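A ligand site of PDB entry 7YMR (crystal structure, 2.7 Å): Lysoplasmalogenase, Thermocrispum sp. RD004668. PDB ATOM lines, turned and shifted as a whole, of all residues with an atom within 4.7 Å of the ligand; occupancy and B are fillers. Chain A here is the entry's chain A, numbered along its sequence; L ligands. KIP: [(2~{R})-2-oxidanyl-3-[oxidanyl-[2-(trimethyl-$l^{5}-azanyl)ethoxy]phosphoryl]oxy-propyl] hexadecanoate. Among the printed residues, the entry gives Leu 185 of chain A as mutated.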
ATOM      1  N   HIS A  20     -21.765   9.619   8.389  1.00  0.00           N
ATOM      2  CA  HIS A  20     -20.686   8.742   8.822  1.00  0.00           C
ATOM      3  C   HIS A  20     -21.233   7.523   9.547  1.00  0.00           C
ATOM      4  O   HIS A  20     -21.698   7.631  10.678  1.00  0.00           O
ATOM      5  CB  HIS A  20     -19.745   9.534   9.730  1.00  0.00           C
ATOM      6  CG  HIS A  20     -18.426   8.867   9.940  1.00  0.00           C
ATOM      7  ND1 HIS A  20     -17.948   8.540  11.188  1.00  0.00           N
ATOM      8  CD2 HIS A  20     -17.485   8.469   9.054  1.00  0.00           C
ATOM      9  CE1 HIS A  20     -16.757   7.974  11.067  1.00  0.00           C
ATOM     10  NE2 HIS A  20     -16.456   7.917   9.779  1.00  0.00           N
ATOM     11  N   ALA A  21     -21.186   6.350   8.920  1.00  0.00           N
ATOM     12  CA  ALA A  21     -21.832   5.159   9.466  1.00  0.00           C
ATOM     13  C   ALA A  21     -23.297   5.406   9.806  1.00  0.00           C
ATOM     14  O   ALA A  21     -23.888   4.662  10.608  1.00  0.00           O
ATOM     15  CB  ALA A  21     -21.091   4.618  10.701  1.00  0.00           C
ATOM     16  N   GLU A  24     -22.775   8.366  13.769  1.00  0.00           N
ATOM     17  CA  GLU A  24     -22.482   7.548  14.935  1.00  0.00           C
ATOM     18  C   GLU A  24     -22.735   8.289  16.254  1.00  0.00           C
ATOM     19  O   GLU A  24     -22.962   7.648  17.275  1.00  0.00           O
ATOM     20  CB  GLU A  24     -21.035   7.015  14.859  1.00  0.00           C
ATOM     21  CG  GLU A  24     -19.927   7.977  15.327  1.00  0.00           C
ATOM     22  CD  GLU A  24     -19.102   8.606  14.195  1.00  0.00           C
ATOM     23  OE1 GLU A  24     -19.572   8.559  13.027  1.00  0.00           O
ATOM     24  OE2 GLU A  24     -18.003   9.161  14.495  1.00  0.00           O
ATOM     25  N   ALA A  29     -24.115   3.320  15.245  1.00  0.00           N
ATOM     26  CA  ALA A  29     -23.358   3.253  13.995  1.00  0.00           C
ATOM     27  C   ALA A  29     -23.669   1.973  13.238  1.00  0.00           C
ATOM     28  O   ALA A  29     -23.931   0.918  13.834  1.00  0.00           O
ATOM     29  CB  ALA A  29     -21.867   3.335  14.285  1.00  0.00           C
ATOM     30  N   GLU A  47     -22.449   6.667   4.401  1.00  0.00           N
ATOM     31  CA  GLU A  47     -21.045   6.284   4.495  1.00  0.00           C
ATOM     32  C   GLU A  47     -21.031   5.088   5.417  1.00  0.00           C
ATOM     33  O   GLU A  47     -21.624   5.141   6.480  1.00  0.00           O
ATOM     34  CB  GLU A  47     -20.187   7.445   5.068  1.00  0.00           C
ATOM     35  CG  GLU A  47     -18.658   7.327   4.948  1.00  0.00           C
ATOM     36  CD  GLU A  47     -18.050   6.353   5.960  1.00  0.00           C
ATOM     37  OE1 GLU A  47     -18.682   6.049   6.999  1.00  0.00           O
ATOM     38  OE2 GLU A  47     -16.928   5.878   5.701  1.00  0.00           O
ATOM     39  N   ASP A  49     -19.043   0.953   6.506  1.00  0.00           N
ATOM     40  CA  ASP A  49     -17.904   0.055   6.575  1.00  0.00           C
ATOM     41  C   ASP A  49     -18.337  -1.397   6.372  1.00  0.00           C
ATOM     42  O   ASP A  49     -19.408  -1.792   6.848  1.00  0.00           O
ATOM     43  CB  ASP A  49     -17.226   0.179   7.917  1.00  0.00           C
ATOM     44  CG  ASP A  49     -17.067   1.611   8.329  1.00  0.00           C
ATOM     45  OD1 ASP A  49     -16.371   2.356   7.617  1.00  0.00           O
ATOM     46  OD2 ASP A  49     -17.666   2.014   9.355  1.00  0.00           O
ATOM     47  N   HIS A  62     -17.774  -1.765  11.518  1.00  0.00           N
ATOM     48  CA  HIS A  62     -16.512  -1.052  11.362  1.00  0.00           C
ATOM     49  C   HIS A  62     -15.332  -1.793  11.975  1.00  0.00           C
ATOM     50  O   HIS A  62     -14.343  -2.062  11.283  1.00  0.00           O
ATOM     51  CB  HIS A  62     -16.608   0.349  11.964  1.00  0.00           C
ATOM     52  CG  HIS A  62     -15.285   1.042  12.079  1.00  0.00           C
ATOM     53  ND1 HIS A  62     -14.402   0.775  13.092  1.00  0.00           N
ATOM     54  CD2 HIS A  62     -14.696   1.967  11.288  1.00  0.00           C
ATOM     55  CE1 HIS A  62     -13.324   1.521  12.940  1.00  0.00           C
ATOM     56  NE2 HIS A  62     -13.488   2.259  11.851  1.00  0.00           N
ATOM     57  N   HIS A  98     -20.821   7.860  20.449  1.00  0.00           N
ATOM     58  CA  HIS A  98     -20.756   6.626  19.670  1.00  0.00           C
ATOM     59  C   HIS A  98     -21.054   5.471  20.626  1.00  0.00           C
ATOM     60  O   HIS A  98     -22.111   5.506  21.275  1.00  0.00           O
ATOM     61  CB  HIS A  98     -19.415   6.597  18.921  1.00  0.00           C
ATOM     62  CG  HIS A  98     -19.152   5.305  18.225  1.00  0.00           C
ATOM     63  ND1 HIS A  98     -20.136   4.600  17.556  1.00  0.00           N
ATOM     64  CD2 HIS A  98     -18.024   4.557  18.134  1.00  0.00           C
ATOM     65  CE1 HIS A  98     -19.624   3.482  17.082  1.00  0.00           C
ATOM     66  NE2 HIS A  98     -18.347   3.423  17.423  1.00  0.00           N
ATOM     67  N   GLU A 149     -16.443   1.457   2.463  1.00  0.00           N
ATOM     68  CA  GLU A 149     -15.044   1.401   2.839  1.00  0.00           C
ATOM     69  C   GLU A 149     -14.683  -0.023   3.218  1.00  0.00           C
ATOM     70  O   GLU A 149     -15.343  -0.631   4.068  1.00  0.00           O
ATOM     71  CB  GLU A 149     -14.756   2.339   3.993  1.00  0.00           C
ATOM     72  CG  GLU A 149     -13.394   2.092   4.581  1.00  0.00           C
ATOM     73  CD  GLU A 149     -12.880   3.289   5.364  1.00  0.00           C
ATOM     74  OE1 GLU A 149     -13.503   4.370   5.267  1.00  0.00           O
ATOM     75  OE2 GLU A 149     -11.874   3.117   6.093  1.00  0.00           O
ATOM     76  N   LYS A 151     -12.770  -2.925   4.984  1.00  0.00           N
ATOM     77  CA  LYS A 151     -12.056  -3.059   6.239  1.00  0.00           C
ATOM     78  C   LYS A 151     -11.387  -4.429   6.283  1.00  0.00           C
ATOM     79  O   LYS A 151     -11.566  -5.260   5.401  1.00  0.00           O
ATOM     80  CB  LYS A 151     -13.014  -2.832   7.410  1.00  0.00           C
ATOM     81  CG  LYS A 151     -13.492  -1.383   7.473  1.00  0.00           C
ATOM     82  CD  LYS A 151     -12.415  -0.487   8.064  1.00  0.00           C
ATOM     83  CE  LYS A 151     -12.911   0.927   8.320  1.00  0.00           C
ATOM     84  NZ  LYS A 151     -11.918   1.768   9.040  1.00  0.00           N
ATOM     85  N   THR A 183     -13.550   2.450  -1.300  1.00  0.00           N
ATOM     86  CA  THR A 183     -12.279   2.949  -0.810  1.00  0.00           C
ATOM     87  C   THR A 183     -11.805   2.037   0.313  1.00  0.00           C
ATOM     88  O   THR A 183     -12.525   1.135   0.742  1.00  0.00           O
ATOM     89  CB  THR A 183     -12.391   4.408  -0.351  1.00  0.00           C
ATOM     90  OG1 THR A 183     -11.087   4.934  -0.057  1.00  0.00           O
ATOM     91  CG2 THR A 183     -13.286   4.526   0.887  1.00  0.00           C
ATOM     92  N   SER A 184     -10.582   2.300   0.769  1.00  0.00           N
ATOM     93  CA  SER A 184      -9.964   1.516   1.840  1.00  0.00           C
ATOM     94  C   SER A 184      -8.752   2.280   2.300  1.00  0.00           C
ATOM     95  O   SER A 184      -8.182   3.040   1.523  1.00  0.00           O
ATOM     96  CB  SER A 184      -9.571   0.117   1.346  1.00  0.00           C
ATOM     97  OG  SER A 184      -8.991  -0.686   2.358  1.00  0.00           O
ATOM     98  N   LEU A 185      -8.355   2.101   3.570  1.00  0.00           N
ATOM     99  CA  LEU A 185      -7.069   2.673   3.940  1.00  0.00           C
ATOM    100  C   LEU A 185      -5.943   1.898   3.273  1.00  0.00           C
ATOM    101  O   LEU A 185      -4.878   2.456   3.038  1.00  0.00           O
ATOM    102  CB  LEU A 185      -6.884   2.742   5.482  1.00  0.00           C
ATOM    103  CG  LEU A 185      -7.889   3.555   6.380  1.00  0.00           C
ATOM    104  CD1 LEU A 185      -8.160   2.951   7.785  1.00  0.00           C
ATOM    105  CD2 LEU A 185      -7.571   5.056   6.564  1.00  0.00           C
ATOM    106  N   PRO A 204      -8.771   7.169  -3.238  1.00  0.00           N
ATOM    107  CA  PRO A 204      -7.470   6.580  -2.925  1.00  0.00           C
ATOM    108  C   PRO A 204      -7.341   6.119  -1.479  1.00  0.00           C
ATOM    109  O   PRO A 204      -7.954   6.664  -0.560  1.00  0.00           O
ATOM    110  CB  PRO A 204      -6.483   7.719  -3.215  1.00  0.00           C
ATOM    111  CG  PRO A 204      -7.292   8.930  -3.333  1.00  0.00           C
ATOM    112  CD  PRO A 204      -8.637   8.514  -3.807  1.00  0.00           C
ATOM    113  N   MET A 206      -4.360   5.102   1.613  1.00  0.00           N
ATOM    114  CA  MET A 206      -3.440   5.921   2.386  1.00  0.00           C
ATOM    115  C   MET A 206      -2.219   6.329   1.554  1.00  0.00           C
ATOM    116  O   MET A 206      -1.828   7.507   1.551  1.00  0.00           O
ATOM    117  CB  MET A 206      -3.004   5.151   3.616  1.00  0.00           C
ATOM    118  CG  MET A 206      -2.093   5.910   4.551  1.00  0.00           C
ATOM    119  SD  MET A 206      -2.226   5.016   6.113  1.00  0.00           S
ATOM    120  CE  MET A 206      -0.934   5.769   7.095  1.00  0.00           C
ATOM    121  N   LEU A 209      -2.895   8.848  -1.149  1.00  0.00           N
ATOM    122  CA  LEU A 209      -3.122  10.197  -0.639  1.00  0.00           C
ATOM    123  C   LEU A 209      -1.803  10.872  -0.334  1.00  0.00           C
ATOM    124  O   LEU A 209      -1.551  12.008  -0.750  1.00  0.00           O
ATOM    125  CB  LEU A 209      -3.998  10.140   0.604  1.00  0.00           C
ATOM    126  CG  LEU A 209      -5.485  10.072   0.331  1.00  0.00           C
ATOM    127  CD1 LEU A 209      -6.216   9.803   1.621  1.00  0.00           C
ATOM    128  CD2 LEU A 209      -5.982  11.355  -0.351  1.00  0.00           C
ATOM    129  N   ALA A 210      -0.945  10.159   0.411  1.00  0.00           N
ATOM    130  CA  ALA A 210       0.398  10.658   0.702  1.00  0.00           C
ATOM    131  C   ALA A 210       1.097  11.053  -0.590  1.00  0.00           C
ATOM    132  O   ALA A 210       1.575  12.176  -0.733  1.00  0.00           O
ATOM    133  CB  ALA A 210       1.204   9.593   1.451  1.00  0.00           C
ATOM    134  N   PHE A 213      -0.444  14.177  -2.079  1.00  0.00           N
ATOM    135  CA  PHE A 213      -0.181  15.378  -1.302  1.00  0.00           C
ATOM    136  C   PHE A 213       1.276  15.792  -1.448  1.00  0.00           C
ATOM    137  O   PHE A 213       1.571  16.967  -1.717  1.00  0.00           O
ATOM    138  CB  PHE A 213      -0.553  15.160   0.175  1.00  0.00           C
ATOM    139  CG  PHE A 213      -0.591  16.435   0.991  1.00  0.00           C
ATOM    140  CD1 PHE A 213       0.580  16.996   1.522  1.00  0.00           C
ATOM    141  CD2 PHE A 213      -1.801  17.070   1.268  1.00  0.00           C
ATOM    142  CE1 PHE A 213       0.546  18.168   2.276  1.00  0.00           C
ATOM    143  CE2 PHE A 213      -1.835  18.242   2.022  1.00  0.00           C
ATOM    144  CZ  PHE A 213      -0.671  18.784   2.524  1.00  0.00           C
ATOM    145  N   LEU A 214       2.181  14.833  -1.331  1.00  0.00           N
ATOM    146  CA  LEU A 214       3.617  15.056  -1.279  1.00  0.00           C
ATOM    147  C   LEU A 214       4.284  15.224  -2.656  1.00  0.00           C
ATOM    148  O   LEU A 214       5.088  16.151  -2.842  1.00  0.00           O
ATOM    149  CB  LEU A 214       4.259  13.882  -0.536  1.00  0.00           C
ATOM    150  CG  LEU A 214       5.730  14.061  -0.298  1.00  0.00           C
ATOM    151  CD1 LEU A 214       5.889  15.270   0.612  1.00  0.00           C
ATOM    152  CD2 LEU A 214       6.348  12.799   0.305  1.00  0.00           C
ATOM    153  N   GLN A 227     -10.806  11.489  -0.316  1.00  0.00           N
ATOM    154  CA  GLN A 227     -11.544  11.405   0.936  1.00  0.00           C
ATOM    155  C   GLN A 227     -10.512  11.480   2.052  1.00  0.00           C
ATOM    156  O   GLN A 227      -9.807  10.497   2.329  1.00  0.00           O
ATOM    157  CB  GLN A 227     -12.383  10.129   0.987  1.00  0.00           C
ATOM    158  CG  GLN A 227     -13.238  10.002  -0.247  1.00  0.00           C
ATOM    159  CD  GLN A 227     -14.374   9.024  -0.119  1.00  0.00           C
ATOM    160  OE1 GLN A 227     -14.274   7.989   0.538  1.00  0.00           O
ATOM    161  NE2 GLN A 227     -15.496   9.383  -0.724  1.00  0.00           N
ATOM    162  N   PRO A 229      -9.113  12.994   6.057  1.00  0.00           N
ATOM    163  CA  PRO A 229      -9.403  13.579   7.368  1.00  0.00           C
ATOM    164  C   PRO A 229      -9.044  15.048   7.338  1.00  0.00           C
ATOM    165  O   PRO A 229      -8.399  15.525   6.389  1.00  0.00           O
ATOM    166  CB  PRO A 229      -8.465  12.824   8.290  1.00  0.00           C
ATOM    167  CG  PRO A 229      -7.271  12.680   7.451  1.00  0.00           C
ATOM    168  CD  PRO A 229      -7.767  12.405   6.042  1.00  0.00           C
ATOM    169  N   TYR A 232      -3.931  15.092   9.894  1.00  0.00           N
ATOM    170  CA  TYR A 232      -3.309  13.804  10.123  1.00  0.00           C
ATOM    171  C   TYR A 232      -1.911  14.012  10.669  1.00  0.00           C
ATOM    172  O   TYR A 232      -1.156  14.820  10.129  1.00  0.00           O
ATOM    173  CB  TYR A 232      -3.250  12.936   8.858  1.00  0.00           C
ATOM    174  CG  TYR A 232      -3.035  11.504   9.246  1.00  0.00           C
ATOM    175  CD1 TYR A 232      -3.892  10.887  10.189  1.00  0.00           C
ATOM    176  CD2 TYR A 232      -1.969  10.755   8.738  1.00  0.00           C
ATOM    177  CE1 TYR A 232      -3.695   9.573  10.589  1.00  0.00           C
ATOM    178  CE2 TYR A 232      -1.777   9.436   9.125  1.00  0.00           C
ATOM    179  CZ  TYR A 232      -2.640   8.853  10.047  1.00  0.00           C
ATOM    180  OH  TYR A 232      -2.475   7.548  10.463  1.00  0.00           O
ATOM    181  N   LEU A 235      -0.421  17.308  10.562  1.00  0.00           N
ATOM    182  CA  LEU A 235      -0.495  18.068   9.324  1.00  0.00           C
ATOM    183  C   LEU A 235      -1.944  18.383   8.991  1.00  0.00           C
ATOM    184  O   LEU A 235      -2.806  17.488   9.005  1.00  0.00           O
ATOM    185  CB  LEU A 235       0.182  17.347   8.164  1.00  0.00           C
ATOM    186  CG  LEU A 235       0.164  18.144   6.839  1.00  0.00           C
ATOM    187  CD1 LEU A 235       0.826  19.550   6.952  1.00  0.00           C
ATOM    188  CD2 LEU A 235       0.827  17.390   5.732  1.00  0.00           C
ATOM    189  N   ILE A 237      -4.711  18.844   6.554  1.00  0.00           N
ATOM    190  CA  ILE A 237      -4.947  18.365   5.196  1.00  0.00           C
ATOM    191  C   ILE A 237      -6.048  19.170   4.516  1.00  0.00           C
ATOM    192  O   ILE A 237      -5.900  19.616   3.383  1.00  0.00           O
ATOM    193  CB  ILE A 237      -5.329  16.868   5.206  1.00  0.00           C
ATOM    194  CG1 ILE A 237      -4.346  16.037   6.030  1.00  0.00           C
ATOM    195  CG2 ILE A 237      -5.385  16.366   3.783  1.00  0.00           C
ATOM    196  CD1 ILE A 237      -2.938  16.050   5.490  1.00  0.00           C
ATOM    197  N   TRP A 256     -13.624  13.866   6.392  1.00  0.00           N
ATOM    198  CA  TRP A 256     -14.142  13.143   7.542  1.00  0.00           C
ATOM    199  C   TRP A 256     -13.402  13.585   8.802  1.00  0.00           C
ATOM    200  O   TRP A 256     -12.510  14.434   8.755  1.00  0.00           O
ATOM    201  CB  TRP A 256     -14.069  11.619   7.320  1.00  0.00           C
ATOM    202  CG  TRP A 256     -12.741  11.071   6.911  1.00  0.00           C
ATOM    203  CD1 TRP A 256     -12.289  10.855   5.621  1.00  0.00           C
ATOM    204  CD2 TRP A 256     -11.693  10.618   7.774  1.00  0.00           C
ATOM    205  NE1 TRP A 256     -11.014  10.331   5.654  1.00  0.00           N
ATOM    206  CE2 TRP A 256     -10.631  10.167   6.955  1.00  0.00           C
ATOM    207  CE3 TRP A 256     -11.545  10.565   9.171  1.00  0.00           C
ATOM    208  CZ2 TRP A 256      -9.456   9.674   7.485  1.00  0.00           C
ATOM    209  CZ3 TRP A 256     -10.380  10.070   9.681  1.00  0.00           C
ATOM    210  CH2 TRP A 256      -9.346   9.633   8.850  1.00  0.00           C
ATOM    211  N   SER A 258     -13.790  11.909  12.797  1.00  0.00           N
ATOM    212  CA  SER A 258     -13.434  10.655  13.446  1.00  0.00           C
ATOM    213  C   SER A 258     -12.166  10.794  14.307  1.00  0.00           C
ATOM    214  O   SER A 258     -11.195  10.052  14.158  1.00  0.00           O
ATOM    215  CB  SER A 258     -13.287   9.552  12.391  1.00  0.00           C
ATOM    216  OG  SER A 258     -13.171   8.274  12.984  1.00  0.00           O
ATOM    217  N   MET A 280     -18.422  14.245   6.138  1.00  0.00           N
ATOM    218  CA  MET A 280     -18.823  12.974   6.718  1.00  0.00           C
ATOM    219  C   MET A 280     -19.035  13.165   8.207  1.00  0.00           C
ATOM    220  O   MET A 280     -18.205  12.746   9.021  1.00  0.00           O
ATOM    221  CB  MET A 280     -17.781  11.894   6.446  1.00  0.00           C
ATOM    222  CG  MET A 280     -17.476  11.674   4.976  1.00  0.00           C
ATOM    223  SD  MET A 280     -16.403  10.248   4.681  1.00  0.00           S
ATOM    224  CE  MET A 280     -15.928  10.563   2.993  1.00  0.00           C
HETATM  225  C10 KIP L   1      -7.368   7.489   4.141  1.00  0.00           C
HETATM  226  C13 KIP L   1      -4.811   9.245   6.496  1.00  0.00           C
HETATM  227  C15 KIP L   1      -3.722  11.156   5.222  1.00  0.00           C
HETATM  228  C17 KIP L   1      -2.344  12.862   3.988  1.00  0.00           C
HETATM  229  C20 KIP L   1       1.403  12.854   3.320  1.00  0.00           C
HETATM  230  C21 KIP L   1       2.646  13.651   3.713  1.00  0.00           C
HETATM  231  C22 KIP L   1     -13.543   6.891   9.062  1.00  0.00           C
HETATM  232  C28 KIP L   1     -14.671   5.669  12.211  1.00  0.00           C
HETATM  233  P24 KIP L   1     -12.319   5.360  10.816  1.00  0.00           P
HETATM  234  C01 KIP L   1     -13.076   7.314   7.648  1.00  0.00           C
HETATM  235  O02 KIP L   1     -14.267   7.435   6.847  1.00  0.00           O
HETATM  236  C03 KIP L   1     -12.089   6.292   6.979  1.00  0.00           C
HETATM  237  O04 KIP L   1     -11.185   6.842   5.925  1.00  0.00           O
HETATM  238  C05 KIP L   1     -11.337   6.644   4.533  1.00  0.00           C
HETATM  239  O06 KIP L   1     -12.255   7.111   3.830  1.00  0.00           O
HETATM  240  C07 KIP L   1     -10.190   5.828   3.845  1.00  0.00           C
HETATM  241  C08 KIP L   1      -9.419   6.709   2.825  1.00  0.00           C
HETATM  242  C09 KIP L   1      -8.749   7.902   3.544  1.00  0.00           C
HETATM  243  C11 KIP L   1      -6.725   8.638   4.987  1.00  0.00           C
HETATM  244  C12 KIP L   1      -5.770   8.122   6.107  1.00  0.00           C
HETATM  245  C14 KIP L   1      -3.980   9.645   5.274  1.00  0.00           C
HETATM  246  C16 KIP L   1      -2.432  11.395   4.439  1.00  0.00           C
HETATM  247  C18 KIP L   1      -1.090  13.043   3.113  1.00  0.00           C
HETATM  248  C19 KIP L   1       0.144  13.514   3.898  1.00  0.00           C
HETATM  249  O23 KIP L   1     -12.456   6.762  10.003  1.00  0.00           O
HETATM  250  O25 KIP L   1     -13.048   4.354   9.979  1.00  0.00           O
HETATM  251  O26 KIP L   1     -10.897   5.095  11.234  1.00  0.00           O
HETATM  252  O27 KIP L   1     -13.205   5.604  12.182  1.00  0.00           O
HETATM  253  C29 KIP L   1     -15.342   4.554  13.059  1.00  0.00           C
HETATM  254  N30 KIP L   1     -16.724   4.901  13.454  1.00  0.00           N
HETATM  255  C31 KIP L   1     -17.552   5.153  12.264  1.00  0.00           C
HETATM  256  C32 KIP L   1     -16.563   6.086  14.366  1.00  0.00           C
HETATM  257  C33 KIP L   1     -17.446   3.769  14.076  1.00  0.00           C
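The side-chain carboxylate (OE2) of Glu 47 is in hydrogen-bond range of an oxygen (O02) of the ligand, at 3.3 Å. A ring nitrogen (NE2) of His 62 is in hydrogen-bond range of an oxygen (O25) of the ligand (2.8 Å). The side-chain amino group (NZ) of Lys 151 is in salt-bridge range of an oxygen (O25) of the ligand (3.0 Å). The side-chain hydroxyl (OG) of Ser 258 sits at hydrogen-bond distance from an oxygen (O27) of the ligand (2.8 Å).
ND1 of His 20 sits at hydrogen-bond distance from OE1 of Glu 24 (2.5 Å). OE2 of Glu 149 is in salt-bridge range of NZ of Lys 151 (3.2 Å). The backbone carbonyl oxygen (O) of Leu 185 sits at hydrogen-bond distance from the backbone NH (N) of Met 206, at 3.0 Å. The backbone carbonyl oxygen (O) of Glu 47 lies within hydrogen-bond range of the backbone NH (N) of Ala 21. A ring nitrogen (NE2) of His 62 lies within hydrogen-bond range of the side-chain amino group (NZ) of Lys 151 (3.3 Å).
An oxygen (O06) of the ligand lies close to the side-chain carboxylate (OE1) of Glu 149. Merely in contact with the ligand: Gln 227 (3.1 Å), His 20 (3.2 Å), Glu 24 (3.4 Å), Leu 185 (3.4 Å), His 98 (3.5 Å), Trp 256 (3.5 Å), Ala 210 (3.6 Å), Ile 237 (3.6 Å), Leu 209 (3.6 Å), Phe 213 (3.7 Å), Pro 204 (3.7 Å), Thr 183 (3.8 Å), Ala 21 (3.9 Å) and Tyr 232 (3.9 Å). Hydrophobic or aromatic side chains within 4 Å of the ligand: His 20, Ala 21, His 62, His 98, Leu 185, Leu 209, Ala 210, Phe 213, Tyr 232, Ile 237 and Trp 256.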
